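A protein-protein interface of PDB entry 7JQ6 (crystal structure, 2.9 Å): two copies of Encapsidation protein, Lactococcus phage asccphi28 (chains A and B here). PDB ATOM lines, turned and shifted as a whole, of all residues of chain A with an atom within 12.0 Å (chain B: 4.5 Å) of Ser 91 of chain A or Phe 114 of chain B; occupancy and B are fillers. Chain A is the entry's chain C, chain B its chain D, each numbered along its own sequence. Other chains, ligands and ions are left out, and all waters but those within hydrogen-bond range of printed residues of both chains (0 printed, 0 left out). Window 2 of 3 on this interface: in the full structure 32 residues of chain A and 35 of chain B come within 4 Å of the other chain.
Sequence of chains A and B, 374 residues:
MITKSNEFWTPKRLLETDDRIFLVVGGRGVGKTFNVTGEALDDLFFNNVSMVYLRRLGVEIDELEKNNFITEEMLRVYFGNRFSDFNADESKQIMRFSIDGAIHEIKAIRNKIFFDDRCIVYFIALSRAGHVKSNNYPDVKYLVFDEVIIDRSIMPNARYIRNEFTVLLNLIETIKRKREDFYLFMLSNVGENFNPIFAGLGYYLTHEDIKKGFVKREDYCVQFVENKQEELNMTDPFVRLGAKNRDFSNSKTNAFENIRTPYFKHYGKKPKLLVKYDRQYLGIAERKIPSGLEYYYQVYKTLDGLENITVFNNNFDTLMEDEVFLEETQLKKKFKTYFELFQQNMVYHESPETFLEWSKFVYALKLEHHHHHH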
ATOM      1  N   GLU A  65     -23.029   6.564 -36.139  1.00  0.00           N
ATOM      2  CA  GLU A  65     -22.161   7.071 -35.076  1.00  0.00           C
ATOM      3  C   GLU A  65     -21.358   5.929 -34.474  1.00  0.00           C
ATOM      4  O   GLU A  65     -21.881   5.126 -33.698  1.00  0.00           O
ATOM      5  CB  GLU A  65     -22.983   7.777 -34.005  1.00  0.00           C
ATOM      6  CG  GLU A  65     -23.530   9.120 -34.434  1.00  0.00           C
ATOM      7  CD  GLU A  65     -22.521  10.241 -34.252  1.00  0.00           C
ATOM      8  OE1 GLU A  65     -21.404   9.963 -33.762  1.00  0.00           O
ATOM      9  OE2 GLU A  65     -22.846  11.399 -34.596  1.00  0.00           O
ATOM     10  N   LYS A  66     -20.076   5.855 -34.829  1.00  0.00           N
ATOM     11  CA  LYS A  66     -19.241   4.764 -34.346  1.00  0.00           C
ATOM     12  C   LYS A  66     -18.977   4.884 -32.850  1.00  0.00           C
ATOM     13  O   LYS A  66     -18.771   3.866 -32.178  1.00  0.00           O
ATOM     14  CB  LYS A  66     -17.923   4.737 -35.120  1.00  0.00           C
ATOM     15  CG  LYS A  66     -18.086   4.443 -36.608  1.00  0.00           C
ATOM     16  N   ASN A  67     -18.991   6.104 -32.306  1.00  0.00           N
ATOM     17  CA  ASN A  67     -18.745   6.270 -30.881  1.00  0.00           C
ATOM     18  C   ASN A  67     -19.949   5.872 -30.036  1.00  0.00           C
ATOM     19  O   ASN A  67     -19.778   5.411 -28.902  1.00  0.00           O
ATOM     20  CB  ASN A  67     -18.366   7.715 -30.565  1.00  0.00           C
ATOM     21  CG  ASN A  67     -17.948   7.898 -29.122  1.00  0.00           C
ATOM     22  OD1 ASN A  67     -17.355   6.999 -28.524  1.00  0.00           O
ATOM     23  ND2 ASN A  67     -18.266   9.053 -28.549  1.00  0.00           N
ATOM     24  N   ASN A  68     -21.161   6.052 -30.556  1.00  0.00           N
ATOM     25  CA  ASN A  68     -22.372   5.686 -29.835  1.00  0.00           C
ATOM     26  C   ASN A  68     -22.866   4.285 -30.178  1.00  0.00           C
ATOM     27  O   ASN A  68     -23.951   3.901 -29.729  1.00  0.00           O
ATOM     28  CB  ASN A  68     -23.490   6.697 -30.111  1.00  0.00           C
ATOM     29  CG  ASN A  68     -23.200   8.063 -29.522  1.00  0.00           C
ATOM     30  OD1 ASN A  68     -22.404   8.194 -28.592  1.00  0.00           O
ATOM     31  ND2 ASN A  68     -23.865   9.089 -30.047  1.00  0.00           N
ATOM     32  N   PHE A  86     -17.063   4.913 -14.773  1.00  0.00           N
ATOM     33  CA  PHE A  86     -16.771   5.069 -16.194  1.00  0.00           C
ATOM     34  C   PHE A  86     -16.528   6.537 -16.516  1.00  0.00           C
ATOM     35  O   PHE A  86     -17.421   7.370 -16.334  1.00  0.00           O
ATOM     36  CB  PHE A  86     -17.930   4.483 -17.012  1.00  0.00           C
ATOM     37  CG  PHE A  86     -17.994   4.948 -18.435  1.00  0.00           C
ATOM     38  CD1 PHE A  86     -17.399   4.213 -19.443  1.00  0.00           C
ATOM     39  CD2 PHE A  86     -18.673   6.107 -18.767  1.00  0.00           C
ATOM     40  CE1 PHE A  86     -17.469   4.631 -20.755  1.00  0.00           C
ATOM     41  CE2 PHE A  86     -18.748   6.530 -20.075  1.00  0.00           C
ATOM     42  CZ  PHE A  86     -18.149   5.790 -21.071  1.00  0.00           C
ATOM     43  N   ASN A  87     -15.313   6.850 -16.993  1.00  0.00           N
ATOM     44  CA  ASN A  87     -14.889   8.224 -17.302  1.00  0.00           C
ATOM     45  C   ASN A  87     -14.231   8.217 -18.683  1.00  0.00           C
ATOM     46  O   ASN A  87     -13.005   8.155 -18.805  1.00  0.00           O
ATOM     47  CB  ASN A  87     -13.952   8.777 -16.227  1.00  0.00           C
ATOM     48  CG  ASN A  87     -14.646   8.974 -14.895  1.00  0.00           C
ATOM     49  OD1 ASN A  87     -14.307   8.334 -13.900  1.00  0.00           O
ATOM     50  ND2 ASN A  87     -15.619   9.878 -14.868  1.00  0.00           N
ATOM     51  N   ALA A  88     -15.059   8.283 -19.719  1.00  0.00           N
ATOM     52  CA  ALA A  88     -14.611   8.247 -21.103  1.00  0.00           C
ATOM     53  C   ALA A  88     -14.323   9.644 -21.645  1.00  0.00           C
ATOM     54  O   ALA A  88     -14.843  10.650 -21.159  1.00  0.00           O
ATOM     55  CB  ALA A  88     -15.659   7.567 -21.982  1.00  0.00           C
ATOM     56  N   ASP A  89     -13.485   9.686 -22.679  1.00  0.00           N
ATOM     57  CA  ASP A  89     -13.163  10.910 -23.409  1.00  0.00           C
ATOM     58  C   ASP A  89     -13.720  10.775 -24.823  1.00  0.00           C
ATOM     59  O   ASP A  89     -13.246   9.952 -25.614  1.00  0.00           O
ATOM     60  CB  ASP A  89     -11.653  11.152 -23.423  1.00  0.00           C
ATOM     61  CG  ASP A  89     -11.228  12.248 -24.399  1.00  0.00           C
ATOM     62  OD1 ASP A  89     -12.102  12.928 -24.976  1.00  0.00           O
ATOM     63  OD2 ASP A  89     -10.005  12.437 -24.581  1.00  0.00           O
ATOM     64  N   GLU A  90     -14.738  11.579 -25.127  1.00  0.00           N
ATOM     65  CA  GLU A  90     -15.426  11.517 -26.404  1.00  0.00           C
ATOM     66  C   GLU A  90     -14.614  12.182 -27.496  1.00  0.00           C
ATOM     67  O   GLU A  90     -14.787  11.877 -28.675  1.00  0.00           O
ATOM     68  CB  GLU A  90     -16.817  12.137 -26.282  1.00  0.00           C
ATOM     69  CG  GLU A  90     -17.757  11.360 -25.371  1.00  0.00           C
ATOM     70  CD  GLU A  90     -19.204  11.788 -25.517  1.00  0.00           C
ATOM     71  OE1 GLU A  90     -19.446  12.888 -26.045  1.00  0.00           O
ATOM     72  OE2 GLU A  90     -20.101  11.021 -25.110  1.00  0.00           O
ATOM     73  N   SER A  91     -13.737  13.121 -27.123  1.00  0.00           N
ATOM     74  CA  SER A  91     -12.971  13.851 -28.129  1.00  0.00           C
ATOM     75  C   SER A  91     -12.200  12.901 -29.027  1.00  0.00           C
ATOM     76  O   SER A  91     -12.245  13.016 -30.255  1.00  0.00           O
ATOM     77  CB  SER A  91     -12.037  14.848 -27.444  1.00  0.00           C
ATOM     78  OG  SER A  91     -11.165  14.184 -26.544  1.00  0.00           O
ATOM     79  N   LYS A  92     -11.474  11.972 -28.440  1.00  0.00           N
ATOM     80  CA  LYS A  92     -10.737  10.956 -29.165  1.00  0.00           C
ATOM     81  C   LYS A  92     -11.519   9.657 -29.318  1.00  0.00           C
ATOM     82  O   LYS A  92     -10.960   8.662 -29.797  1.00  0.00           O
ATOM     83  CB  LYS A  92      -9.398  10.723 -28.489  1.00  0.00           C
ATOM     84  CG  LYS A  92      -8.521  11.975 -28.418  1.00  0.00           C
ATOM     85  CD  LYS A  92      -7.185  11.703 -27.731  1.00  0.00           C
ATOM     86  CE  LYS A  92      -6.289  10.808 -28.584  1.00  0.00           C
ATOM     87  NZ  LYS A  92      -4.917  10.651 -28.015  1.00  0.00           N
ATOM     88  N   GLN A  93     -12.774   9.628 -28.868  1.00  0.00           N
ATOM     89  CA  GLN A  93     -13.625   8.445 -28.989  1.00  0.00           C
ATOM     90  C   GLN A  93     -13.019   7.254 -28.256  1.00  0.00           C
ATOM     91  O   GLN A  93     -13.000   6.132 -28.764  1.00  0.00           O
ATOM     92  CB  GLN A  93     -13.896   8.109 -30.455  1.00  0.00           C
ATOM     93  CG  GLN A  93     -14.740   9.159 -31.166  1.00  0.00           C
ATOM     94  CD  GLN A  93     -14.880   8.902 -32.652  1.00  0.00           C
ATOM     95  OE1 GLN A  93     -15.992   8.821 -33.179  1.00  0.00           O
ATOM     96  NE2 GLN A  93     -13.750   8.786 -33.340  1.00  0.00           N
ATOM     97  N   ILE A  94     -12.510   7.503 -27.051  1.00  0.00           N
ATOM     98  CA  ILE A  94     -11.890   6.476 -26.223  1.00  0.00           C
ATOM     99  C   ILE A  94     -12.702   6.356 -24.941  1.00  0.00           C
ATOM    100  O   ILE A  94     -12.951   7.361 -24.264  1.00  0.00           O
ATOM    101  CB  ILE A  94     -10.418   6.801 -25.905  1.00  0.00           C
ATOM    102  CG1 ILE A  94      -9.600   6.872 -27.200  1.00  0.00           C
ATOM    103  CG2 ILE A  94      -9.830   5.751 -24.957  1.00  0.00           C
ATOM    104  CD1 ILE A  94      -8.133   7.233 -27.002  1.00  0.00           C
ATOM    105  N   MET A  95     -13.124   5.136 -24.622  1.00  0.00           N
ATOM    106  CA  MET A  95     -13.810   4.856 -23.367  1.00  0.00           C
ATOM    107  C   MET A  95     -12.889   4.057 -22.452  1.00  0.00           C
ATOM    108  O   MET A  95     -12.204   3.142 -22.906  1.00  0.00           O
ATOM    109  CB  MET A  95     -15.106   4.073 -23.602  1.00  0.00           C
ATOM    110  CG  MET A  95     -16.235   4.861 -24.265  1.00  0.00           C
ATOM    111  SD  MET A  95     -17.917   3.849 -24.345  1.00  0.00           S
ATOM    112  CE  MET A  95     -19.072   5.213 -25.129  1.00  0.00           C
ATOM    113  N   ARG A  96     -12.868   4.414 -21.170  1.00  0.00           N
ATOM    114  CA  ARG A  96     -12.178   3.640 -20.146  1.00  0.00           C
ATOM    115  C   ARG A  96     -13.157   3.244 -19.053  1.00  0.00           C
ATOM    116  O   ARG A  96     -13.880   4.092 -18.517  1.00  0.00           O
ATOM    117  CB  ARG A  96     -10.991   4.394 -19.539  1.00  0.00           C
ATOM    118  CG  ARG A  96      -9.790   4.497 -20.462  1.00  0.00           C
ATOM    119  CD  ARG A  96      -8.578   5.055 -19.731  1.00  0.00           C
ATOM    120  NE  ARG A  96      -7.376   5.055 -20.564  1.00  0.00           N
ATOM    121  CZ  ARG A  96      -7.020   6.037 -21.390  1.00  0.00           C
ATOM    122  NH1 ARG A  96      -7.771   7.125 -21.509  1.00  0.00           N
ATOM    123  NH2 ARG A  96      -5.904   5.929 -22.100  1.00  0.00           N
ATOM    124  N   GLU A 105     -10.065  -0.566 -22.179  1.00  0.00           N
ATOM    125  CA  GLU A 105     -10.429   0.604 -22.969  1.00  0.00           C
ATOM    126  C   GLU A 105     -10.851   0.186 -24.371  1.00  0.00           C
ATOM    127  O   GLU A 105     -10.223  -0.681 -24.987  1.00  0.00           O
ATOM    128  CB  GLU A 105      -9.282   1.633 -23.079  1.00  0.00           C
ATOM    129  CG  GLU A 105      -8.152   1.283 -24.053  1.00  0.00           C
ATOM    130  CD  GLU A 105      -7.186   2.446 -24.268  1.00  0.00           C
ATOM    131  OE1 GLU A 105      -7.304   3.461 -23.549  1.00  0.00           O
ATOM    132  OE2 GLU A 105      -6.312   2.350 -25.155  1.00  0.00           O
ATOM    133  N   ILE A 106     -11.913   0.813 -24.867  1.00  0.00           N
ATOM    134  CA  ILE A 106     -12.382   0.626 -26.237  1.00  0.00           C
ATOM    135  C   ILE A 106     -12.291   1.967 -26.952  1.00  0.00           C
ATOM    136  O   ILE A 106     -12.906   2.949 -26.520  1.00  0.00           O
ATOM    137  CB  ILE A 106     -13.816   0.075 -26.288  1.00  0.00           C
ATOM    138  CG1 ILE A 106     -14.772   0.955 -25.479  1.00  0.00           C
ATOM    139  CG2 ILE A 106     -13.852  -1.357 -25.780  1.00  0.00           C
ATOM    140  CD1 ILE A 106     -16.196   0.429 -25.428  1.00  0.00           C
ATOM    141  N   LYS A 107     -11.533   2.011 -28.044  1.00  0.00           N
ATOM    142  CA  LYS A 107     -11.388   3.221 -28.842  1.00  0.00           C
ATOM    143  C   LYS A 107     -11.909   2.959 -30.249  1.00  0.00           C
ATOM    144  O   LYS A 107     -11.557   1.951 -30.869  1.00  0.00           O
ATOM    145  CB  LYS A 107      -9.929   3.689 -28.885  1.00  0.00           C
ATOM    146  CG  LYS A 107      -8.958   2.722 -29.540  1.00  0.00           C
ATOM    147  CD  LYS A 107      -7.532   3.266 -29.518  1.00  0.00           C
ATOM    148  CE  LYS A 107      -6.945   3.247 -28.111  1.00  0.00           C
ATOM    149  NZ  LYS A 107      -5.564   3.805 -28.051  1.00  0.00           N
ATOM    150  N   ALA A 108     -12.752   3.866 -30.741  1.00  0.00           N
ATOM    151  CA  ALA A 108     -13.365   3.747 -32.057  1.00  0.00           C
ATOM    152  C   ALA A 108     -12.709   4.750 -32.994  1.00  0.00           C
ATOM    153  O   ALA A 108     -12.770   5.960 -32.752  1.00  0.00           O
ATOM    154  CB  ALA A 108     -14.873   3.989 -31.985  1.00  0.00           C
ATOM    155  N   ILE A 109     -12.075   4.246 -34.050  1.00  0.00           N
ATOM    156  CA  ILE A 109     -11.428   5.080 -35.055  1.00  0.00           C
ATOM    157  C   ILE A 109     -11.847   4.564 -36.426  1.00  0.00           C
ATOM    158  O   ILE A 109     -11.848   3.351 -36.663  1.00  0.00           O
ATOM    159  CB  ILE A 109      -9.895   5.081 -34.909  1.00  0.00           C
ATOM    160  CG1 ILE A 109      -9.310   3.683 -35.098  1.00  0.00           C
ATOM    161  CG2 ILE A 109      -9.496   5.595 -33.530  1.00  0.00           C
ATOM    162  CD1 ILE A 109      -8.914   3.381 -36.536  1.00  0.00           C
ATOM    163  N   ARG A 110     -12.209   5.479 -37.321  1.00  0.00           N
ATOM    164  CA  ARG A 110     -12.634   5.138 -38.689  1.00  0.00           C
ATOM    165  C   ARG A 110     -13.811   4.169 -38.590  1.00  0.00           C
ATOM    166  O   ARG A 110     -14.775   4.459 -37.862  1.00  0.00           O
ATOM    167  CB  ARG A 110     -11.437   4.609 -39.475  1.00  0.00           C
ATOM    168  CG  ARG A 110     -10.358   5.614 -39.827  1.00  0.00           C
ATOM    169  CD  ARG A 110      -9.278   4.950 -40.686  1.00  0.00           C
ATOM    170  NE  ARG A 110      -9.814   4.359 -41.918  1.00  0.00           N
ATOM    171  CZ  ARG A 110     -10.261   3.107 -42.042  1.00  0.00           C
ATOM    172  NH1 ARG A 110     -10.256   2.277 -41.005  1.00  0.00           N
ATOM    173  NH2 ARG A 110     -10.726   2.684 -43.210  1.00  0.00           N
ATOM    174  N   GLU B 105     -12.037  23.965 -21.875  1.00  0.00           N
ATOM    175  CA  GLU B 105     -11.666  24.178 -23.268  1.00  0.00           C
ATOM    176  C   GLU B 105     -12.723  23.616 -24.205  1.00  0.00           C
ATOM    177  O   GLU B 105     -13.302  22.559 -23.944  1.00  0.00           O
ATOM    178  CB  GLU B 105     -10.290  23.561 -23.586  1.00  0.00           C
ATOM    179  CG  GLU B 105     -10.260  22.050 -23.743  1.00  0.00           C
ATOM    180  CD  GLU B 105      -8.908  21.556 -24.228  1.00  0.00           C
ATOM    181  OE1 GLU B 105      -7.961  22.376 -24.277  1.00  0.00           O
ATOM    182  OE2 GLU B 105      -8.793  20.351 -24.549  1.00  0.00           O
ATOM    183  N   ILE B 106     -12.971  24.335 -25.297  1.00  0.00           N
ATOM    184  CA  ILE B 106     -13.879  23.898 -26.351  1.00  0.00           C
ATOM    185  C   ILE B 106     -13.064  23.671 -27.617  1.00  0.00           C
ATOM    186  O   ILE B 106     -12.273  24.535 -28.017  1.00  0.00           O
ATOM    187  CB  ILE B 106     -14.996  24.925 -26.602  1.00  0.00           C
ATOM    188  CG1 ILE B 106     -15.808  25.147 -25.331  1.00  0.00           C
ATOM    189  CG2 ILE B 106     -15.915  24.456 -27.724  1.00  0.00           C
ATOM    190  CD1 ILE B 106     -16.982  26.081 -25.518  1.00  0.00           C
ATOM    191  N   LYS B 107     -13.257  22.512 -28.247  1.00  0.00           N
ATOM    192  CA  LYS B 107     -12.604  22.178 -29.507  1.00  0.00           C
ATOM    193  C   LYS B 107     -13.650  21.631 -30.465  1.00  0.00           C
ATOM    194  O   LYS B 107     -14.439  20.756 -30.095  1.00  0.00           O
ATOM    195  CB  LYS B 107     -11.477  21.156 -29.304  1.00  0.00           C
ATOM    196  CG  LYS B 107     -11.936  19.824 -28.734  1.00  0.00           C
ATOM    197  CD  LYS B 107     -10.765  18.948 -28.292  1.00  0.00           C
ATOM    198  CE  LYS B 107     -10.184  19.408 -26.956  1.00  0.00           C
ATOM    199  NZ  LYS B 107      -9.148  18.468 -26.433  1.00  0.00           N
ATOM    200  N   ILE B 109     -14.416  19.577 -33.785  1.00  0.00           N
ATOM    201  CA  ILE B 109     -13.860  18.574 -34.683  1.00  0.00           C
ATOM    202  C   ILE B 109     -14.999  17.951 -35.474  1.00  0.00           C
ATOM    203  O   ILE B 109     -16.020  17.561 -34.897  1.00  0.00           O
ATOM    204  CB  ILE B 109     -13.092  17.483 -33.911  1.00  0.00           C
ATOM    205  CG1 ILE B 109     -11.773  18.040 -33.373  1.00  0.00           C
ATOM    206  CG2 ILE B 109     -12.862  16.263 -34.799  1.00  0.00           C
ATOM    207  CD1 ILE B 109     -11.087  17.125 -32.372  1.00  0.00           C
ATOM    208  N   LYS B 112     -18.954  17.764 -34.662  1.00  0.00           N
ATOM    209  CA  LYS B 112     -19.172  17.737 -33.227  1.00  0.00           C
ATOM    210  C   LYS B 112     -18.386  18.864 -32.579  1.00  0.00           C
ATOM    211  O   LYS B 112     -17.311  19.241 -33.052  1.00  0.00           O
ATOM    212  CB  LYS B 112     -18.719  16.389 -32.662  1.00  0.00           C
ATOM    213  CG  LYS B 112     -19.466  15.215 -33.276  1.00  0.00           C
ATOM    214  CD  LYS B 112     -18.897  13.869 -32.866  1.00  0.00           C
ATOM    215  CE  LYS B 112     -19.548  12.755 -33.677  1.00  0.00           C
ATOM    216  NZ  LYS B 112     -18.913  11.427 -33.432  1.00  0.00           N
ATOM    217  N   ILE B 113     -18.931  19.395 -31.489  1.00  0.00           N
ATOM    218  CA  ILE B 113     -18.240  20.368 -30.652  1.00  0.00           C
ATOM    219  C   ILE B 113     -18.005  19.717 -29.296  1.00  0.00           C
ATOM    220  O   ILE B 113     -18.923  19.121 -28.720  1.00  0.00           O
ATOM    221  CB  ILE B 113     -19.039  21.674 -30.519  1.00  0.00           C
ATOM    222  CG1 ILE B 113     -19.138  22.352 -31.887  1.00  0.00           C
ATOM    223  CG2 ILE B 113     -18.369  22.597 -29.515  1.00  0.00           C
ATOM    224  CD1 ILE B 113     -19.868  23.686 -31.878  1.00  0.00           C
ATOM    225  N   PHE B 114     -16.779  19.819 -28.797  1.00  0.00           N
ATOM    226  CA  PHE B 114     -16.362  19.158 -27.567  1.00  0.00           C
ATOM    227  C   PHE B 114     -16.059  20.199 -26.498  1.00  0.00           C
ATOM    228  O   PHE B 114     -15.352  21.176 -26.761  1.00  0.00           O
ATOM    229  CB  PHE B 114     -15.136  18.296 -27.857  1.00  0.00           C
ATOM    230  CG  PHE B 114     -15.407  17.149 -28.796  1.00  0.00           C
ATOM    231  CD1 PHE B 114     -14.641  16.982 -29.936  1.00  0.00           C
ATOM    232  CD2 PHE B 114     -16.472  16.291 -28.587  1.00  0.00           C
ATOM    233  CE1 PHE B 114     -14.897  15.948 -30.818  1.00  0.00           C
ATOM    234  CE2 PHE B 114     -16.721  15.247 -29.457  1.00  0.00           C
ATOM    235  CZ  PHE B 114     -15.940  15.083 -30.578  1.00  0.00           C
ATOM    236  N   PHE B 115     -16.590  19.981 -25.294  1.00  0.00           N
ATOM    237  CA  PHE B 115     -16.328  20.832 -24.136  1.00  0.00           C
ATOM    238  C   PHE B 115     -15.637  19.987 -23.076  1.00  0.00           C
ATOM    239  O   PHE B 115     -16.234  19.049 -22.538  1.00  0.00           O
ATOM    240  CB  PHE B 115     -17.616  21.433 -23.584  1.00  0.00           C
ATOM    241  CG  PHE B 115     -17.439  22.129 -22.264  1.00  0.00           C
ATOM    242  CD1 PHE B 115     -16.977  23.434 -22.213  1.00  0.00           C
ATOM    243  CD2 PHE B 115     -17.717  21.476 -21.075  1.00  0.00           C
ATOM    244  CE1 PHE B 115     -16.811  24.078 -21.003  1.00  0.00           C
ATOM    245  CE2 PHE B 115     -17.548  22.113 -19.863  1.00  0.00           C
ATOM    246  CZ  PHE B 115     -17.094  23.416 -19.826  1.00  0.00           C
ATOM    247  N   ASP B 116     -14.382  20.310 -22.776  1.00  0.00           N
ATOM    248  CA  ASP B 116     -13.589  19.513 -21.847  1.00  0.00           C
ATOM    249  C   ASP B 116     -13.585  18.058 -22.301  1.00  0.00           C
ATOM    250  O   ASP B 116     -13.787  17.128 -21.518  1.00  0.00           O
ATOM    251  CB  ASP B 116     -14.101  19.638 -20.413  1.00  0.00           C
ATOM    252  CG  ASP B 116     -13.627  20.903 -19.734  1.00  0.00           C
ATOM    253  OD1 ASP B 116     -12.925  21.701 -20.388  1.00  0.00           O
ATOM    254  OD2 ASP B 116     -13.945  21.093 -18.541  1.00  0.00           O
ATOM    255  N   ASP B 117     -13.369  17.871 -23.599  1.00  0.00           N
ATOM    256  CA  ASP B 117     -13.287  16.551 -24.209  1.00  0.00           C
ATOM    257  C   ASP B 117     -14.615  15.800 -24.165  1.00  0.00           C
ATOM    258  O   ASP B 117     -14.634  14.573 -24.303  1.00  0.00           O
ATOM    259  CB  ASP B 117     -12.186  15.723 -23.536  1.00  0.00           C
ATOM    260  CG  ASP B 117     -10.802  16.309 -23.757  1.00  0.00           C
ATOM    261  OD1 ASP B 117     -10.708  17.443 -24.274  1.00  0.00           O
ATOM    262  OD2 ASP B 117      -9.810  15.634 -23.412  1.00  0.00           O
ATOM    263  N   ARG B 118     -15.730  16.508 -23.987  1.00  0.00           N
ATOM    264  CA  ARG B 118     -17.062  15.911 -23.982  1.00  0.00           C
ATOM    265  C   ARG B 118     -17.926  16.581 -25.046  1.00  0.00           C
ATOM    266  O   ARG B 118     -17.916  17.808 -25.182  1.00  0.00           O
ATOM    267  CB  ARG B 118     -17.722  16.056 -22.607  1.00  0.00           C
ATOM    268  CG  ARG B 118     -19.041  15.325 -22.472  1.00  0.00           C
ATOM    269  CD  ARG B 118     -19.609  15.475 -21.072  1.00  0.00           C
ATOM    270  NE  ARG B 118     -19.843  16.875 -20.728  1.00  0.00           N
ATOM    271  CZ  ARG B 118     -20.959  17.539 -21.018  1.00  0.00           C
ATOM    272  NH1 ARG B 118     -21.954  16.935 -21.658  1.00  0.00           N
ATOM    273  NH2 ARG B 118     -21.082  18.810 -20.667  1.00  0.00           N
ATOM    274  N   CYS B 119     -18.685  15.774 -25.790  1.00  0.00           N
ATOM    275  CA  CYS B 119     -19.465  16.272 -26.919  1.00  0.00           C
ATOM    276  C   CYS B 119     -20.711  16.998 -26.429  1.00  0.00           C
ATOM    277  O   CYS B 119     -21.560  16.403 -25.757  1.00  0.00           O
ATOM    278  CB  CYS B 119     -19.855  15.122 -27.844  1.00  0.00           C
ATOM    279  SG  CYS B 119     -20.810  15.603 -29.305  1.00  0.00           S
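The side-chain carboxylate (OE1) of Glu 65 of chain A is in salt-bridge range of the side-chain amino group (NZ) of Lys 112 of chain B (2.9 Å).
O of Asp 117 of chain B lies within hydrogen-bond range of N of Glu 90 of chain A.
The side-chain carboxylate (OE1) of Glu 90 of chain A sits close to the backbone NH (N) of Cys 119 of chain B, 3.0 Å away.
O of Asp 117 of chain B is in hydrogen-bond range of N of Ser 91 of chain A (3.3 Å).
The backbone carbonyl oxygen (O) of Asp 117 of chain B lies close to the side-chain carboxylate (OD1) of Asp 89 of chain A (3.1 Å).
OD1 of Asp 89 of chain A lies within hydrogen-bond range of N of Ser 91 of chain A (2.7 Å).
The backbone NH (N) of Asp 89 of chain A is in hydrogen-bond range of the backbone carbonyl oxygen (O) of Ile 94 of chain A (2.9 Å).
The backbone carbonyl oxygen (O) of Gln 93 of chain A lies within hydrogen-bond range of the backbone NH (N) of Ala 108 of chain A, 3.0 Å away.
The backbone carbonyl oxygen (O) of Lys 107 of chain B is in hydrogen-bond range of the backbone NH (N) of Phe 114 of chain B.
NZ of Lys 107 of chain B lies within salt-bridge range of OD1 of Asp 117 of chain B, 2.9 Å away.
Among the printed residues, pairs that only touch across the chains: Glu 90 of chain A with Phe 114 of chain B, Ser 91 of chain A with Phe 114 of chain B and Gln 93 of chain A with Lys 112 of chain B.
Printed residues of chain B within 4 Å of Ser 91 of chain A: Phe 114 (3.9 Å) and Asp 117 (3.3 Å).
Of chain A, only Glu 90 and Ser 91 come within 4 Å of Phe 114 of chain B.
No residue of chain A comes within 4 Å of Ile 106 of chain B.
Lys 107 of chain B touches none of the printed residues of chain A.
No residue of chain A comes within 4 Å of Ile 109 of chain B.
Lys 112 of chain B touches just these residues of chain A: Glu 65 (2.9 Å) and Gln 93 (3.9 Å).
Ile 113 of chain B touches none of the printed residues of chain A.
Printed residues of chain A within 4 Å of Asp 117 of chain B: Asp 89, Glu 90 and Ser 91.
Cys 119 of chain B touches just one residue of chain A: Glu 90 (2.9 Å).
Of the printed residues of chain B, Glu 65 of chain A touches Lys 112 (2.9 Å).
Of the printed residues of chain B, Gln 93 of chain A touches Lys 112.
Of the printed residues of chain B, Asp 89 of chain A touches Asp 117.
Of the printed residues of chain B, Glu 90 of chain A touches Phe 114, Asp 117 and Cys 119.
Ala 108 of chain A touches none of the printed residues of chain B.
Arg 118 of chain B touches none of the printed residues of chain A.
The nearest printed residue of chain B that does not touch Asp 89 of chain A is Arg 118 of chain B (5.2 Å).
Hydrophobic or aromatic side chains of chain B that line the printed part of chain A: Phe 114.
Printed residues of chain A that touch a printed residue of chain B: Glu 65, Asp 89, Glu 90, Ser 91 and Gln 93.
Along chain A the printed residues that touch a printed residue of chain B span positions 65 to 93.
4 positions are printed for both chains.
Of the 8 pairs that touch across the chains among the printed residues, none has its exchanged pair printed and touching as well.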
